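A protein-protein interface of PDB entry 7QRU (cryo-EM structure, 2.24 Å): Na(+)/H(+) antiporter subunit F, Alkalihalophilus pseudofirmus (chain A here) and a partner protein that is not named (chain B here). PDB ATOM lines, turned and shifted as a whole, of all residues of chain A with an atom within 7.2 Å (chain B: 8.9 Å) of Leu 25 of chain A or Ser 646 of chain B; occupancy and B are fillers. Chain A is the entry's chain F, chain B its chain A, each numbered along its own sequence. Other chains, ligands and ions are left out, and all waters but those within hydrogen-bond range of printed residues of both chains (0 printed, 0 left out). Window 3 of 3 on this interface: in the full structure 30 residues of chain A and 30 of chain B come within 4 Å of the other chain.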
ATOM      1  N   CYS A  20      36.043   9.558 -33.819  1.00  0.00           N
ATOM      2  CA  CYS A  20      34.865   9.851 -34.635  1.00  0.00           C
ATOM      3  C   CYS A  20      33.536   9.807 -33.884  1.00  0.00           C
ATOM      4  O   CYS A  20      32.570  10.423 -34.286  1.00  0.00           O
ATOM      5  CB  CYS A  20      34.679   8.875 -35.791  1.00  0.00           C
ATOM      6  SG  CYS A  20      35.989   9.054 -36.985  1.00  0.00           S
ATOM      7  N   PHE A  21      33.339   8.801 -33.067  1.00  0.00           N
ATOM      8  CA  PHE A  21      32.125   8.700 -32.291  1.00  0.00           C
ATOM      9  C   PHE A  21      31.872   9.966 -31.433  1.00  0.00           C
ATOM     10  O   PHE A  21      30.757  10.330 -31.203  1.00  0.00           O
ATOM     11  CB  PHE A  21      32.214   7.417 -31.454  1.00  0.00           C
ATOM     12  CG  PHE A  21      31.193   7.382 -30.386  1.00  0.00           C
ATOM     13  CD1 PHE A  21      29.848   7.219 -30.716  1.00  0.00           C
ATOM     14  CD2 PHE A  21      31.579   7.584 -29.071  1.00  0.00           C
ATOM     15  CE1 PHE A  21      28.886   7.263 -29.720  1.00  0.00           C
ATOM     16  CE2 PHE A  21      30.619   7.541 -28.070  1.00  0.00           C
ATOM     17  CZ  PHE A  21      29.274   7.458 -28.402  1.00  0.00           C
ATOM     18  N   ILE A  22      32.873  10.623 -30.901  1.00  0.00           N
ATOM     19  CA  ILE A  22      32.618  11.771 -30.058  1.00  0.00           C
ATOM     20  C   ILE A  22      31.825  12.833 -30.824  1.00  0.00           C
ATOM     21  O   ILE A  22      30.902  13.450 -30.261  1.00  0.00           O
ATOM     22  CB  ILE A  22      33.964  12.395 -29.560  1.00  0.00           C
ATOM     23  CG1 ILE A  22      34.818  11.468 -28.685  1.00  0.00           C
ATOM     24  CG2 ILE A  22      33.746  13.658 -28.791  1.00  0.00           C
ATOM     25  CD1 ILE A  22      33.927  10.696 -27.735  1.00  0.00           C
ATOM     26  N   ARG A  23      32.128  13.084 -32.109  1.00  0.00           N
ATOM     27  CA  ARG A  23      31.378  14.111 -32.819  1.00  0.00           C
ATOM     28  C   ARG A  23      29.986  13.642 -33.189  1.00  0.00           C
ATOM     29  O   ARG A  23      29.132  14.503 -33.370  1.00  0.00           O
ATOM     30  CB  ARG A  23      32.128  14.648 -34.023  1.00  0.00           C
ATOM     31  CG  ARG A  23      33.098  15.753 -33.606  1.00  0.00           C
ATOM     32  CD  ARG A  23      32.863  16.901 -34.496  1.00  0.00           C
ATOM     33  NE  ARG A  23      33.893  17.881 -34.222  1.00  0.00           N
ATOM     34  CZ  ARG A  23      33.836  18.771 -33.241  1.00  0.00           C
ATOM     35  NH1 ARG A  23      32.807  18.832 -32.437  1.00  0.00           N
ATOM     36  NH2 ARG A  23      34.850  19.581 -33.037  1.00  0.00           N
ATOM     37  N   THR A  24      29.743  12.331 -33.291  1.00  0.00           N
ATOM     38  CA  THR A  24      28.375  11.883 -33.536  1.00  0.00           C
ATOM     39  C   THR A  24      27.496  12.240 -32.341  1.00  0.00           C
ATOM     40  O   THR A  24      26.338  12.570 -32.558  1.00  0.00           O
ATOM     41  CB  THR A  24      28.229  10.396 -33.860  1.00  0.00           C
ATOM     42  OG1 THR A  24      28.560   9.748 -32.628  1.00  0.00           O
ATOM     43  CG2 THR A  24      29.074   9.914 -35.021  1.00  0.00           C
ATOM     44  N   LEU A  25      28.075  12.325 -31.150  1.00  0.00           N
ATOM     45  CA  LEU A  25      27.367  12.747 -29.957  1.00  0.00           C
ATOM     46  C   LEU A  25      27.299  14.242 -29.851  1.00  0.00           C
ATOM     47  O   LEU A  25      26.204  14.772 -29.702  1.00  0.00           O
ATOM     48  CB  LEU A  25      28.046  12.206 -28.684  1.00  0.00           C
ATOM     49  CG  LEU A  25      27.640  10.787 -28.369  1.00  0.00           C
ATOM     50  CD1 LEU A  25      28.226  10.436 -27.052  1.00  0.00           C
ATOM     51  CD2 LEU A  25      26.116  10.754 -28.377  1.00  0.00           C
ATOM     52  N   ILE A  26      28.451  14.866 -29.824  1.00  0.00           N
ATOM     53  CA  ILE A  26      28.472  16.283 -29.505  1.00  0.00           C
ATOM     54  C   ILE A  26      28.224  17.213 -30.729  1.00  0.00           C
ATOM     55  O   ILE A  26      28.034  18.406 -30.510  1.00  0.00           O
ATOM     56  CB  ILE A  26      29.821  16.666 -28.828  1.00  0.00           C
ATOM     57  CG1 ILE A  26      30.999  16.740 -29.784  1.00  0.00           C
ATOM     58  CG2 ILE A  26      30.151  15.707 -27.760  1.00  0.00           C
ATOM     59  CD1 ILE A  26      32.145  17.351 -29.197  1.00  0.00           C
ATOM     60  N   GLY A  27      28.229  16.759 -31.998  1.00  0.00           N
ATOM     61  CA  GLY A  27      27.891  17.649 -33.107  1.00  0.00           C
ATOM     62  C   GLY A  27      29.012  18.667 -33.217  1.00  0.00           C
ATOM     63  O   GLY A  27      30.199  18.260 -33.199  1.00  0.00           O
ATOM     64  N   PRO A  28      28.748  19.991 -33.211  1.00  0.00           N
ATOM     65  CA  PRO A  28      27.503  20.633 -32.775  1.00  0.00           C
ATOM     66  C   PRO A  28      26.273  20.572 -33.659  1.00  0.00           C
ATOM     67  O   PRO A  28      25.150  20.637 -33.169  1.00  0.00           O
ATOM     68  CB  PRO A  28      27.765  22.146 -32.766  1.00  0.00           C
ATOM     69  CG  PRO A  28      29.024  22.258 -33.476  1.00  0.00           C
ATOM     70  CD  PRO A  28      29.792  20.964 -33.432  1.00  0.00           C
ATOM     71  N   ARG A  33      27.555  15.587 -37.249  1.00  0.00           N
ATOM     72  CA  ARG A  33      27.275  14.232 -36.890  1.00  0.00           C
ATOM     73  C   ARG A  33      27.290  13.279 -38.095  1.00  0.00           C
ATOM     74  O   ARG A  33      27.678  12.119 -37.912  1.00  0.00           O
ATOM     75  CB  ARG A  33      25.903  14.177 -36.186  1.00  0.00           C
ATOM     76  CG  ARG A  33      25.918  15.021 -34.930  1.00  0.00           C
ATOM     77  CD  ARG A  33      24.692  14.652 -34.169  1.00  0.00           C
ATOM     78  NE  ARG A  33      24.895  15.090 -32.800  1.00  0.00           N
ATOM     79  CZ  ARG A  33      24.609  16.311 -32.409  1.00  0.00           C
ATOM     80  NH1 ARG A  33      23.809  17.051 -33.136  1.00  0.00           N
ATOM     81  NH2 ARG A  33      24.924  16.705 -31.201  1.00  0.00           N
ATOM     82  N   ALA A  36      30.991  12.755 -39.106  1.00  0.00           N
ATOM     83  CA  ALA A  36      31.608  11.804 -38.223  1.00  0.00           C
ATOM     84  C   ALA A  36      31.104  10.436 -38.554  1.00  0.00           C
ATOM     85  O   ALA A  36      31.906   9.565 -38.559  1.00  0.00           O
ATOM     86  CB  ALA A  36      31.307  12.148 -36.836  1.00  0.00           C
ATOM     87  N   VAL B 639      33.514   1.790 -26.869  1.00  0.00           N
ATOM     88  CA  VAL B 639      32.706   2.660 -27.718  1.00  0.00           C
ATOM     89  C   VAL B 639      31.279   2.134 -27.775  1.00  0.00           C
ATOM     90  O   VAL B 639      30.313   2.872 -27.948  1.00  0.00           O
ATOM     91  CB  VAL B 639      33.273   2.784 -29.154  1.00  0.00           C
ATOM     92  CG1 VAL B 639      32.408   3.624 -30.098  1.00  0.00           C
ATOM     93  CG2 VAL B 639      34.666   3.370 -29.096  1.00  0.00           C
ATOM     94  N   PHE B 640      31.161   0.847 -27.906  1.00  0.00           N
ATOM     95  CA  PHE B 640      29.861   0.240 -28.078  1.00  0.00           C
ATOM     96  C   PHE B 640      28.976   0.548 -26.863  1.00  0.00           C
ATOM     97  O   PHE B 640      27.794   0.913 -26.996  1.00  0.00           O
ATOM     98  CB  PHE B 640      30.075  -1.251 -28.292  1.00  0.00           C
ATOM     99  CG  PHE B 640      28.822  -1.967 -28.659  1.00  0.00           C
ATOM    100  CD1 PHE B 640      27.945  -2.382 -27.692  1.00  0.00           C
ATOM    101  CD2 PHE B 640      28.459  -2.118 -29.980  1.00  0.00           C
ATOM    102  CE1 PHE B 640      26.743  -2.965 -28.051  1.00  0.00           C
ATOM    103  CE2 PHE B 640      27.297  -2.773 -30.338  1.00  0.00           C
ATOM    104  CZ  PHE B 640      26.430  -3.175 -29.364  1.00  0.00           C
ATOM    105  N   ILE B 641      29.581   0.464 -25.693  1.00  0.00           N
ATOM    106  CA  ILE B 641      28.892   0.734 -24.447  1.00  0.00           C
ATOM    107  C   ILE B 641      28.616   2.209 -24.315  1.00  0.00           C
ATOM    108  O   ILE B 641      27.463   2.536 -24.049  1.00  0.00           O
ATOM    109  CB  ILE B 641      29.639   0.134 -23.215  1.00  0.00           C
ATOM    110  CG1 ILE B 641      29.499  -1.366 -23.274  1.00  0.00           C
ATOM    111  CG2 ILE B 641      29.120   0.647 -21.916  1.00  0.00           C
ATOM    112  CD1 ILE B 641      30.520  -2.070 -22.478  1.00  0.00           C
ATOM    113  N   ALA B 642      29.614   3.089 -24.482  1.00  0.00           N
ATOM    114  CA  ALA B 642      29.306   4.526 -24.535  1.00  0.00           C
ATOM    115  C   ALA B 642      28.204   4.881 -25.532  1.00  0.00           C
ATOM    116  O   ALA B 642      27.281   5.607 -25.179  1.00  0.00           O
ATOM    117  CB  ALA B 642      30.509   5.279 -24.875  1.00  0.00           C
ATOM    118  N   ALA B 643      28.235   4.346 -26.764  1.00  0.00           N
ATOM    119  CA  ALA B 643      27.204   4.735 -27.719  1.00  0.00           C
ATOM    120  C   ALA B 643      25.824   4.335 -27.208  1.00  0.00           C
ATOM    121  O   ALA B 643      24.899   5.114 -27.195  1.00  0.00           O
ATOM    122  CB  ALA B 643      27.429   4.115 -29.061  1.00  0.00           C
ATOM    123  N   THR B 644      25.739   3.102 -26.717  1.00  0.00           N
ATOM    124  CA  THR B 644      24.518   2.595 -26.160  1.00  0.00           C
ATOM    125  C   THR B 644      24.026   3.391 -24.940  1.00  0.00           C
ATOM    126  O   THR B 644      22.837   3.644 -24.858  1.00  0.00           O
ATOM    127  CB  THR B 644      24.695   1.121 -25.733  1.00  0.00           C
ATOM    128  OG1 THR B 644      25.169   0.353 -26.839  1.00  0.00           O
ATOM    129  CG2 THR B 644      23.363   0.591 -25.271  1.00  0.00           C
ATOM    130  N   LEU B 645      24.872   3.716 -23.955  1.00  0.00           N
ATOM    131  CA  LEU B 645      24.435   4.532 -22.838  1.00  0.00           C
ATOM    132  C   LEU B 645      24.043   5.957 -23.212  1.00  0.00           C
ATOM    133  O   LEU B 645      23.448   6.624 -22.417  1.00  0.00           O
ATOM    134  CB  LEU B 645      25.524   4.614 -21.801  1.00  0.00           C
ATOM    135  CG  LEU B 645      25.686   3.276 -21.087  1.00  0.00           C
ATOM    136  CD1 LEU B 645      26.977   3.253 -20.367  1.00  0.00           C
ATOM    137  CD2 LEU B 645      24.543   3.001 -20.121  1.00  0.00           C
ATOM    138  N   SER B 646      24.462   6.488 -24.313  1.00  0.00           N
ATOM    139  CA  SER B 646      24.129   7.861 -24.664  1.00  0.00           C
ATOM    140  C   SER B 646      22.686   7.909 -25.155  1.00  0.00           C
ATOM    141  O   SER B 646      22.002   8.870 -25.029  1.00  0.00           O
ATOM    142  CB  SER B 646      25.127   8.288 -25.726  1.00  0.00           C
ATOM    143  OG  SER B 646      24.687   7.805 -27.039  1.00  0.00           O
ATOM    144  N   ILE B 647      22.128   6.806 -25.625  1.00  0.00           N
ATOM    145  CA  ILE B 647      20.850   6.959 -26.264  1.00  0.00           C
ATOM    146  C   ILE B 647      19.806   7.588 -25.379  1.00  0.00           C
ATOM    147  O   ILE B 647      19.085   8.410 -25.885  1.00  0.00           O
ATOM    148  CB  ILE B 647      20.368   5.646 -26.861  1.00  0.00           C
ATOM    149  CG1 ILE B 647      21.379   5.280 -27.950  1.00  0.00           C
ATOM    150  CG2 ILE B 647      18.981   5.856 -27.465  1.00  0.00           C
ATOM    151  CD1 ILE B 647      21.383   3.892 -28.204  1.00  0.00           C
ATOM    152  N   PRO B 648      19.553   7.190 -24.118  1.00  0.00           N
ATOM    153  CA  PRO B 648      18.518   7.864 -23.348  1.00  0.00           C
ATOM    154  C   PRO B 648      18.764   9.346 -23.126  1.00  0.00           C
ATOM    155  O   PRO B 648      17.827  10.022 -22.794  1.00  0.00           O
ATOM    156  CB  PRO B 648      18.605   7.189 -22.005  1.00  0.00           C
ATOM    157  CG  PRO B 648      19.169   5.929 -22.295  1.00  0.00           C
ATOM    158  CD  PRO B 648      20.201   6.143 -23.334  1.00  0.00           C
ATOM    159  N   PHE B 649      19.951   9.889 -23.425  1.00  0.00           N
ATOM    160  CA  PHE B 649      20.120  11.315 -23.207  1.00  0.00           C
ATOM    161  C   PHE B 649      20.004  12.125 -24.466  1.00  0.00           C
ATOM    162  O   PHE B 649      20.138  13.329 -24.430  1.00  0.00           O
ATOM    163  CB  PHE B 649      21.515  11.591 -22.729  1.00  0.00           C
ATOM    164  CG  PHE B 649      21.844  10.895 -21.465  1.00  0.00           C
ATOM    165  CD1 PHE B 649      21.497  11.476 -20.274  1.00  0.00           C
ATOM    166  CD2 PHE B 649      22.307   9.589 -21.478  1.00  0.00           C
ATOM    167  CE1 PHE B 649      21.777  10.811 -19.081  1.00  0.00           C
ATOM    168  CE2 PHE B 649      22.535   8.905 -20.282  1.00  0.00           C
ATOM    169  CZ  PHE B 649      22.274   9.530 -19.085  1.00  0.00           C
ATOM    170  N   ILE B 650      19.717  11.486 -25.569  1.00  0.00           N
ATOM    171  CA  ILE B 650      19.634  12.215 -26.800  1.00  0.00           C
ATOM    172  C   ILE B 650      18.251  12.817 -26.959  1.00  0.00           C
ATOM    173  O   ILE B 650      17.346  12.049 -26.978  1.00  0.00           O
ATOM    174  CB  ILE B 650      19.907  11.223 -27.954  1.00  0.00           C
ATOM    175  CG1 ILE B 650      21.372  10.854 -27.912  1.00  0.00           C
ATOM    176  CG2 ILE B 650      19.470  11.739 -29.326  1.00  0.00           C
ATOM    177  CD1 ILE B 650      21.644   9.699 -28.782  1.00  0.00           C
ATOM    178  N   ASN B 651      18.111  14.061 -27.416  1.00  0.00           N
ATOM    179  CA  ASN B 651      16.808  14.651 -27.632  1.00  0.00           C
ATOM    180  C   ASN B 651      16.503  15.164 -29.027  1.00  0.00           C
ATOM    181  O   ASN B 651      15.522  15.896 -29.237  1.00  0.00           O
ATOM    182  CB  ASN B 651      16.599  15.887 -26.747  1.00  0.00           C
ATOM    183  CG  ASN B 651      16.988  15.572 -25.334  1.00  0.00           C
ATOM    184  OD1 ASN B 651      17.856  16.240 -24.775  1.00  0.00           O
ATOM    185  ND2 ASN B 651      16.416  14.504 -24.811  1.00  0.00           N
ATOM    186  N   LYS B 652      17.290  14.800 -29.975  1.00  0.00           N
ATOM    187  CA  LYS B 652      17.023  15.150 -31.341  1.00  0.00           C
ATOM    188  C   LYS B 652      16.973  13.855 -32.096  1.00  0.00           C
ATOM    189  O   LYS B 652      17.873  13.042 -31.824  1.00  0.00           O
ATOM    190  CB  LYS B 652      18.231  15.892 -31.880  1.00  0.00           C
ATOM    191  CG  LYS B 652      18.393  17.223 -31.186  1.00  0.00           C
ATOM    192  CD  LYS B 652      17.530  18.272 -31.746  1.00  0.00           C
ATOM    193  CE  LYS B 652      17.525  19.491 -30.856  1.00  0.00           C
ATOM    194  NZ  LYS B 652      16.265  20.252 -31.025  1.00  0.00           N
ATOM    195  N   THR B 655      20.077  12.765 -34.272  1.00  0.00           N
ATOM    196  CA  THR B 655      21.175  12.254 -33.496  1.00  0.00           C
ATOM    197  C   THR B 655      20.889  10.782 -33.144  1.00  0.00           C
ATOM    198  O   THR B 655      21.758   9.928 -33.128  1.00  0.00           O
ATOM    199  CB  THR B 655      21.366  13.052 -32.221  1.00  0.00           C
ATOM    200  OG1 THR B 655      21.697  14.382 -32.523  1.00  0.00           O
ATOM    201  CG2 THR B 655      22.475  12.446 -31.391  1.00  0.00           C
ATOM    202  N   ALA B 656      19.648  10.483 -32.827  1.00  0.00           N
ATOM    203  CA  ALA B 656      19.297   9.148 -32.420  1.00  0.00           C
ATOM    204  C   ALA B 656      19.635   8.198 -33.589  1.00  0.00           C
ATOM    205  O   ALA B 656      20.190   7.125 -33.410  1.00  0.00           O
ATOM    206  CB  ALA B 656      17.851   9.100 -32.029  1.00  0.00           C
ATOM    207  N   VAL B 658      21.777   8.526 -36.082  1.00  0.00           N
ATOM    208  CA  VAL B 658      23.214   8.400 -36.204  1.00  0.00           C
ATOM    209  C   VAL B 658      23.831   7.467 -35.159  1.00  0.00           C
ATOM    210  O   VAL B 658      24.641   6.637 -35.510  1.00  0.00           O
ATOM    211  CB  VAL B 658      23.896   9.776 -36.174  1.00  0.00           C
ATOM    212  CG1 VAL B 658      25.374   9.688 -36.085  1.00  0.00           C
ATOM    213  CG2 VAL B 658      23.508  10.565 -37.431  1.00  0.00           C
ATOM    214  N   VAL B 659      23.428   7.557 -33.904  1.00  0.00           N
ATOM    215  CA  VAL B 659      23.995   6.733 -32.877  1.00  0.00           C
ATOM    216  C   VAL B 659      23.470   5.309 -32.931  1.00  0.00           C
ATOM    217  O   VAL B 659      24.252   4.365 -32.713  1.00  0.00           O
ATOM    218  CB  VAL B 659      23.850   7.399 -31.499  1.00  0.00           C
ATOM    219  CG1 VAL B 659      24.366   6.556 -30.396  1.00  0.00           C
ATOM    220  CG2 VAL B 659      24.644   8.714 -31.516  1.00  0.00           C
ATOM    221  N   VAL B 660      22.293   5.125 -33.448  1.00  0.00           N
ATOM    222  CA  VAL B 660      21.848   3.801 -33.798  1.00  0.00           C
ATOM    223  C   VAL B 660      22.676   3.175 -34.932  1.00  0.00           C
ATOM    224  O   VAL B 660      22.921   1.984 -34.880  1.00  0.00           O
ATOM    225  CB  VAL B 660      20.327   3.808 -34.059  1.00  0.00           C
ATOM    226  CG1 VAL B 660      19.835   2.557 -34.721  1.00  0.00           C
ATOM    227  CG2 VAL B 660      19.655   3.985 -32.717  1.00  0.00           C
ATOM    228  N   VAL B 662      25.849   4.010 -35.533  1.00  0.00           N
ATOM    229  CA  VAL B 662      27.081   3.641 -34.931  1.00  0.00           C
ATOM    230  C   VAL B 662      26.910   2.259 -34.323  1.00  0.00           C
ATOM    231  O   VAL B 662      27.820   1.419 -34.426  1.00  0.00           O
ATOM    232  CB  VAL B 662      27.613   4.672 -33.923  1.00  0.00           C
ATOM    233  CG1 VAL B 662      28.752   4.078 -33.113  1.00  0.00           C
ATOM    234  CG2 VAL B 662      27.991   5.903 -34.695  1.00  0.00           C
ATOM    235  N   ILE B 663      25.871   2.079 -33.532  1.00  0.00           N
ATOM    236  CA  ILE B 663      25.710   0.820 -32.805  1.00  0.00           C
ATOM    237  C   ILE B 663      25.620  -0.346 -33.791  1.00  0.00           C
ATOM    238  O   ILE B 663      26.260  -1.401 -33.599  1.00  0.00           O
ATOM    239  CB  ILE B 663      24.513   0.885 -31.811  1.00  0.00           C
ATOM    240  CG1 ILE B 663      24.966   1.632 -30.544  1.00  0.00           C
ATOM    241  CG2 ILE B 663      24.049  -0.488 -31.451  1.00  0.00           C
ATOM    242  CD1 ILE B 663      23.852   2.380 -29.885  1.00  0.00           C
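Of chain B, only Val 658 (3.7 Å) comes within 4 Å of Thr 24 of chain A. Of chain B, only Ser 646 comes within 4 Å of Leu 25 of chain A. Printed residues of chain B within 4 Å of Arg 33 of chain A: Thr 655 and Val 658. Of the printed residues of chain A, Val 639 of chain B touches Phe 21. Printed residues of chain A within 4 Å of Ala 642 of chain B: Phe 21. Printed residues of chain A within 4 Å of Thr 655 of chain B: Arg 33 (3.3 Å). Of the printed residues of chain A, Val 658 of chain B touches Thr 24 (3.7 Å) and Arg 33 (3.8 Å). The nearest residue of chain A that does not touch Ser 646 of chain B is Phe 21 of chain A (4.8 Å). The nearest printed residue of chain A that does not touch Ala 643 of chain B is Leu 25 of chain A (5.8 Å).
Of the 11 printed residues of chain A, 4 touch a printed residue of chain B. Hydrophobic or aromatic side chains of chain A that line the printed part of chain B: Phe 21 and Leu 25. Of the 21 printed residues of chain B, 6 touch a printed residue of chain A. Among the printed residues, 7 pairs touch across the chains. Among the printed residues, no Asp or Glu carboxylate lies within 4 Å of a Lys or Arg side-chain nitrogen of the other chain.
Phe 21 of chain A touches Val 639 of chain B (CG to CG1, 3.96 Å). CB of Ala 642 of chain B touches CE2 of Phe 21 of chain A (3.9 Å). CZ of Phe 21 of chain A touches CA of Ala 643 of chain B (3.5 Å). Val 658 of chain B touches Thr 24 of chain A. Ser 646 of chain B touches Leu 25 of chain A. Arg 33 of chain A touches Val 658 of chain B (O to CG1, 3.8 Å).
The side-chain hydroxyl (OG1) of Thr 655 of chain B is in hydrogen-bond range of the guanidinium group (NE) of Arg 33 of chain A, at 3.3 Å.
The backbone carbonyl oxygen (O) of Ala 643 of chain B lies within hydrogen-bond range of the side-chain hydroxyl (OG) of Ser 646 of chain B, 2.7 Å away. The backbone carbonyl oxygen (O) of Phe 21 of chain A sits at hydrogen-bond distance from the side-chain hydroxyl (OG1) of Thr 24 of chain A, 2.7 Å away. NE of Arg 33 of chain A sits at hydrogen-bond distance from O of Thr 24 of chain A, 2.9 Å away. O of Leu 25 of chain A lies within hydrogen-bond range of NH2 of Arg 33 of chain A, at 2.8 Å.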
